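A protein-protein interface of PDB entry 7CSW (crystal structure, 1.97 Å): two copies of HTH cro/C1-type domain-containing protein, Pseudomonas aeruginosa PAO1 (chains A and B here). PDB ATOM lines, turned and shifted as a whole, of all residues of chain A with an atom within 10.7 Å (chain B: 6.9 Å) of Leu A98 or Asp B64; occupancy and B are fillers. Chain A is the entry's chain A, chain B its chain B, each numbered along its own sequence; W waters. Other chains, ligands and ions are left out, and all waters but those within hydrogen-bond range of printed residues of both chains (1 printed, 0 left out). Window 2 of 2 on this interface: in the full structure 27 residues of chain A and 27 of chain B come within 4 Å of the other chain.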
ATOM      1  N   ILE A  94      -6.884  31.652  -3.067  1.00  0.00           N
ATOM      2  CA  ILE A  94      -6.572  31.021  -4.348  1.00  0.00           C
ATOM      3  C   ILE A  94      -7.075  31.903  -5.481  1.00  0.00           C
ATOM      4  O   ILE A  94      -8.284  32.104  -5.625  1.00  0.00           O
ATOM      5  CB  ILE A  94      -7.187  29.620  -4.465  1.00  0.00           C
ATOM      6  CG1 ILE A  94      -6.687  28.702  -3.337  1.00  0.00           C
ATOM      7  CG2 ILE A  94      -6.905  29.038  -5.855  1.00  0.00           C
ATOM      8  CD1 ILE A  94      -7.084  27.212  -3.518  1.00  0.00           C
ATOM      9  N   GLU A  95      -6.148  32.388  -6.327  1.00  0.00           N
ATOM     10  CA  GLU A  95      -6.595  33.073  -7.533  1.00  0.00           C
ATOM     11  C   GLU A  95      -6.804  32.063  -8.659  1.00  0.00           C
ATOM     12  O   GLU A  95      -5.904  31.268  -8.940  1.00  0.00           O
ATOM     13  CB  GLU A  95      -5.585  34.124  -7.974  1.00  0.00           C
ATOM     14  CG  GLU A  95      -5.905  34.716  -9.345  1.00  0.00           C
ATOM     15  CD  GLU A  95      -5.177  36.019  -9.624  1.00  0.00           C
ATOM     16  OE1 GLU A  95      -5.840  36.988 -10.068  1.00  0.00           O
ATOM     17  OE2 GLU A  95      -3.948  36.071  -9.409  1.00  0.00           O
ATOM     18  N   PRO A  96      -7.950  32.074  -9.333  1.00  0.00           N
ATOM     19  CA  PRO A  96      -8.180  31.095 -10.402  1.00  0.00           C
ATOM     20  C   PRO A  96      -7.163  31.257 -11.520  1.00  0.00           C
ATOM     21  O   PRO A  96      -6.659  32.353 -11.781  1.00  0.00           O
ATOM     22  CB  PRO A  96      -9.597  31.417 -10.887  1.00  0.00           C
ATOM     23  CG  PRO A  96     -10.175  32.324  -9.847  1.00  0.00           C
ATOM     24  CD  PRO A  96      -9.059  33.028  -9.197  1.00  0.00           C
ATOM     25  N   LEU A  97      -6.872  30.136 -12.185  1.00  0.00           N
ATOM     26  CA  LEU A  97      -5.859  30.132 -13.234  1.00  0.00           C
ATOM     27  C   LEU A  97      -6.201  31.097 -14.362  1.00  0.00           C
ATOM     28  O   LEU A  97      -5.294  31.692 -14.957  1.00  0.00           O
ATOM     29  CB  LEU A  97      -5.688  28.719 -13.775  1.00  0.00           C
ATOM     30  CG  LEU A  97      -4.493  28.447 -14.686  1.00  0.00           C
ATOM     31  CD1 LEU A  97      -3.219  28.959 -14.041  1.00  0.00           C
ATOM     32  CD2 LEU A  97      -4.418  26.953 -14.966  1.00  0.00           C
ATOM     33  N   LEU A  98      -7.482  31.266 -14.686  1.00  0.00           N
ATOM     34  CA  LEU A  98      -7.835  32.250 -15.704  1.00  0.00           C
ATOM     35  C   LEU A  98      -7.344  33.631 -15.268  1.00  0.00           C
ATOM     36  O   LEU A  98      -7.609  34.066 -14.144  1.00  0.00           O
ATOM     37  CB  LEU A  98      -9.340  32.227 -15.975  1.00  0.00           C
ATOM     38  CG  LEU A  98     -10.393  32.373 -14.873  1.00  0.00           C
ATOM     39  CD1 LEU A  98     -10.800  33.824 -14.642  1.00  0.00           C
ATOM     40  CD2 LEU A  98     -11.603  31.524 -15.208  1.00  0.00           C
ATOM     41  N   ALA A  99      -6.577  34.277 -16.151  1.00  0.00           N
ATOM     42  CA  ALA A  99      -5.730  35.446 -15.857  1.00  0.00           C
ATOM     43  C   ALA A  99      -4.512  35.075 -14.997  1.00  0.00           C
ATOM     44  O   ALA A  99      -3.358  35.155 -15.456  1.00  0.00           O
ATOM     45  CB  ALA A  99      -6.536  36.561 -15.189  1.00  0.00           C
ATOM     46  N   PHE B  19      -5.040  17.866 -16.256  1.00  0.00           N
ATOM     47  CA  PHE B  19      -4.814  19.241 -15.822  1.00  0.00           C
ATOM     48  C   PHE B  19      -3.331  19.553 -15.691  1.00  0.00           C
ATOM     49  O   PHE B  19      -2.819  20.448 -16.376  1.00  0.00           O
ATOM     50  CB  PHE B  19      -5.556  19.510 -14.504  1.00  0.00           C
ATOM     51  CG  PHE B  19      -7.056  19.510 -14.654  1.00  0.00           C
ATOM     52  CD1 PHE B  19      -7.748  20.692 -14.842  1.00  0.00           C
ATOM     53  CD2 PHE B  19      -7.767  18.322 -14.642  1.00  0.00           C
ATOM     54  CE1 PHE B  19      -9.130  20.690 -15.002  1.00  0.00           C
ATOM     55  CE2 PHE B  19      -9.145  18.313 -14.805  1.00  0.00           C
ATOM     56  CZ  PHE B  19      -9.828  19.501 -14.981  1.00  0.00           C
ATOM     57  N   ARG B  58     -10.671  23.549  -3.548  1.00  0.00           N
ATOM     58  CA  ARG B  58      -9.460  24.215  -4.034  1.00  0.00           C
ATOM     59  C   ARG B  58      -9.204  23.915  -5.501  1.00  0.00           C
ATOM     60  O   ARG B  58      -8.819  24.809  -6.265  1.00  0.00           O
ATOM     61  CB  ARG B  58      -8.249  23.793  -3.211  1.00  0.00           C
ATOM     62  CG  ARG B  58      -8.448  23.984  -1.724  1.00  0.00           C
ATOM     63  CD  ARG B  58      -7.213  23.589  -0.931  1.00  0.00           C
ATOM     64  NE  ARG B  58      -6.567  24.796  -0.462  1.00  0.00           N
ATOM     65  CZ  ARG B  58      -6.803  25.370   0.710  1.00  0.00           C
ATOM     66  NH1 ARG B  58      -7.643  24.838   1.569  1.00  0.00           N
ATOM     67  NH2 ARG B  58      -6.175  26.485   1.008  1.00  0.00           N
ATOM     68  N   LEU B  59      -9.351  22.652  -5.904  1.00  0.00           N
ATOM     69  CA  LEU B  59      -9.087  22.305  -7.294  1.00  0.00           C
ATOM     70  C   LEU B  59     -10.123  22.931  -8.216  1.00  0.00           C
ATOM     71  O   LEU B  59      -9.777  23.453  -9.277  1.00  0.00           O
ATOM     72  CB  LEU B  59      -9.074  20.788  -7.463  1.00  0.00           C
ATOM     73  CG  LEU B  59      -7.923  20.065  -6.773  1.00  0.00           C
ATOM     74  CD1 LEU B  59      -8.181  18.560  -6.754  1.00  0.00           C
ATOM     75  CD2 LEU B  59      -6.622  20.379  -7.487  1.00  0.00           C
ATOM     76  N   GLY B  60     -11.401  22.864  -7.837  1.00  0.00           N
ATOM     77  CA  GLY B  60     -12.425  23.510  -8.639  1.00  0.00           C
ATOM     78  C   GLY B  60     -12.151  24.991  -8.800  1.00  0.00           C
ATOM     79  O   GLY B  60     -12.261  25.538  -9.899  1.00  0.00           O
ATOM     80  N   ARG B  61     -11.737  25.639  -7.711  1.00  0.00           N
ATOM     81  CA  ARG B  61     -11.507  27.079  -7.708  1.00  0.00           C
ATOM     82  C   ARG B  61     -10.330  27.453  -8.608  1.00  0.00           C
ATOM     83  O   ARG B  61     -10.427  28.376  -9.425  1.00  0.00           O
ATOM     84  CB  ARG B  61     -11.271  27.534  -6.267  1.00  0.00           C
ATOM     85  CG  ARG B  61     -10.600  28.881  -6.096  1.00  0.00           C
ATOM     86  CD  ARG B  61     -11.471  29.974  -6.648  1.00  0.00           C
ATOM     87  NE  ARG B  61     -11.154  31.300  -6.118  1.00  0.00           N
ATOM     88  CZ  ARG B  61     -11.911  32.367  -6.363  1.00  0.00           C
ATOM     89  NH1 ARG B  61     -11.601  33.567  -5.869  1.00  0.00           N
ATOM     90  NH2 ARG B  61     -12.990  32.221  -7.115  1.00  0.00           N
ATOM     91  N   TYR B  62      -9.217  26.726  -8.484  1.00  0.00           N
ATOM     92  CA  TYR B  62      -8.010  27.055  -9.238  1.00  0.00           C
ATOM     93  C   TYR B  62      -8.160  26.717 -10.712  1.00  0.00           C
ATOM     94  O   TYR B  62      -7.799  27.520 -11.583  1.00  0.00           O
ATOM     95  CB  TYR B  62      -6.806  26.318  -8.653  1.00  0.00           C
ATOM     96  CG  TYR B  62      -5.492  26.685  -9.330  1.00  0.00           C
ATOM     97  CD1 TYR B  62      -5.006  27.988  -9.285  1.00  0.00           C
ATOM     98  CD2 TYR B  62      -4.748  25.731 -10.018  1.00  0.00           C
ATOM     99  CE1 TYR B  62      -3.797  28.333  -9.910  1.00  0.00           C
ATOM    100  CE2 TYR B  62      -3.536  26.068 -10.645  1.00  0.00           C
ATOM    101  CZ  TYR B  62      -3.072  27.369 -10.583  1.00  0.00           C
ATOM    102  OH  TYR B  62      -1.880  27.709 -11.198  1.00  0.00           O
ATOM    103  N   PHE B  63      -8.674  25.525 -11.022  1.00  0.00           N
ATOM    104  CA  PHE B  63      -8.767  25.066 -12.402  1.00  0.00           C
ATOM    105  C   PHE B  63     -10.082  25.448 -13.088  1.00  0.00           C
ATOM    106  O   PHE B  63     -10.350  24.955 -14.190  1.00  0.00           O
ATOM    107  CB  PHE B  63      -8.574  23.548 -12.464  1.00  0.00           C
ATOM    108  CG  PHE B  63      -7.131  23.117 -12.310  1.00  0.00           C
ATOM    109  CD1 PHE B  63      -6.155  23.591 -13.185  1.00  0.00           C
ATOM    110  CD2 PHE B  63      -6.756  22.263 -11.295  1.00  0.00           C
ATOM    111  CE1 PHE B  63      -4.822  23.209 -13.059  1.00  0.00           C
ATOM    112  CE2 PHE B  63      -5.418  21.869 -11.154  1.00  0.00           C
ATOM    113  CZ  PHE B  63      -4.449  22.356 -12.050  1.00  0.00           C
ATOM    114  N   ASP B  64     -10.905  26.297 -12.473  1.00  0.00           N
ATOM    115  CA  ASP B  64     -12.193  26.671 -13.062  1.00  0.00           C
ATOM    116  C   ASP B  64     -12.991  25.425 -13.460  1.00  0.00           C
ATOM    117  O   ASP B  64     -13.380  25.244 -14.615  1.00  0.00           O
ATOM    118  CB  ASP B  64     -11.984  27.614 -14.259  1.00  0.00           C
ATOM    119  CG  ASP B  64     -13.294  28.174 -14.827  1.00  0.00           C
ATOM    120  OD1 ASP B  64     -14.187  28.547 -14.023  1.00  0.00           O
ATOM    121  OD2 ASP B  64     -13.419  28.251 -16.085  1.00  0.00           O
ATOM    122  N   THR B  65     -13.185  24.521 -12.500  1.00  0.00           N
ATOM    123  CA  THR B  65     -14.065  23.373 -12.686  1.00  0.00           C
ATOM    124  C   THR B  65     -15.124  23.381 -11.591  1.00  0.00           C
ATOM    125  O   THR B  65     -15.031  24.115 -10.601  1.00  0.00           O
ATOM    126  CB  THR B  65     -13.312  22.025 -12.658  1.00  0.00           C
ATOM    127  OG1 THR B  65     -13.031  21.659 -11.299  1.00  0.00           O
ATOM    128  CG2 THR B  65     -11.989  22.079 -13.436  1.00  0.00           C
ATOM    129  N   SER B  66     -16.154  22.566 -11.804  1.00  0.00           N
ATOM    130  CA  SER B  66     -17.072  22.201 -10.730  1.00  0.00           C
ATOM    131  C   SER B  66     -16.288  21.624  -9.555  1.00  0.00           C
ATOM    132  O   SER B  66     -15.371  20.817  -9.741  1.00  0.00           O
ATOM    133  CB  SER B  66     -18.078  21.176 -11.254  1.00  0.00           C
ATOM    134  OG  SER B  66     -18.835  20.613 -10.197  1.00  0.00           O
HETATM  135  O   HOH W   1      -8.918  28.992 -13.762  1.00  0.00           O
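Among the printed residues, merely in contact across the chains: Ile A94 with Arg B58, Ile A94 with Tyr B62, Glu A95 with Tyr B62, Pro A96 with Arg B61, Pro A96 with Tyr B62 and Leu A98 with Asp B64.
The guanidinium group (NE) of Arg B61 is in hydrogen-bond range of the backbone carbonyl oxygen (O) of Ile A94 (3.0 Å).
The backbone carbonyl oxygen (O) of Tyr B62 sits at hydrogen-bond distance from the backbone NH (N) of Leu A97, at 2.8 Å.
Of the 6 printed residues of chain A, 5 touch a printed residue of chain B.
Hydrophobic or aromatic side chains of chain B that line the printed part of chain A: Tyr B62.
Water W1 lies within hydrogen-bond range of the backbone NH (N) of Leu A97 (2.8 Å), the backbone NH (N) of Leu A98 (2.8 Å) and the backbone carbonyl oxygen (O) of Tyr B62 (2.9 Å).
Printed residues of chain B within 4 Å of Ile A94: Arg B58, Arg B61 and Tyr B62.
Of the printed residues of chain B, Pro A96 touches Arg B61 (3.5 Å) and Tyr B62 (3.8 Å).
Of the printed residues of chain B, Leu A97 touches Tyr B62 (2.8 Å).
Of chain B, only Asp B64 comes within 4 Å of Leu A98.
No residue of chain A comes within 4 Å of Gly B60.
Of the printed residues of chain A, Arg B61 touches Ile A94 (3.0 Å) and Pro A96 (3.5 Å).
Of the printed residues of chain A, Tyr B62 touches Ile A94, Glu A95, Pro A96 and Leu A97.
Asp B64 touches just one residue of chain A: Leu A98 (3.8 Å).
No residue of chain A comes within 4 Å of Thr B65.
The nearest residue of chain B that does not touch Leu A98 is Tyr B62 (4.9 Å).
No position is printed for both chains.
Of the 8 pairs that touch across the chains among the printed residues, none has its exchanged pair printed and touching as well.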
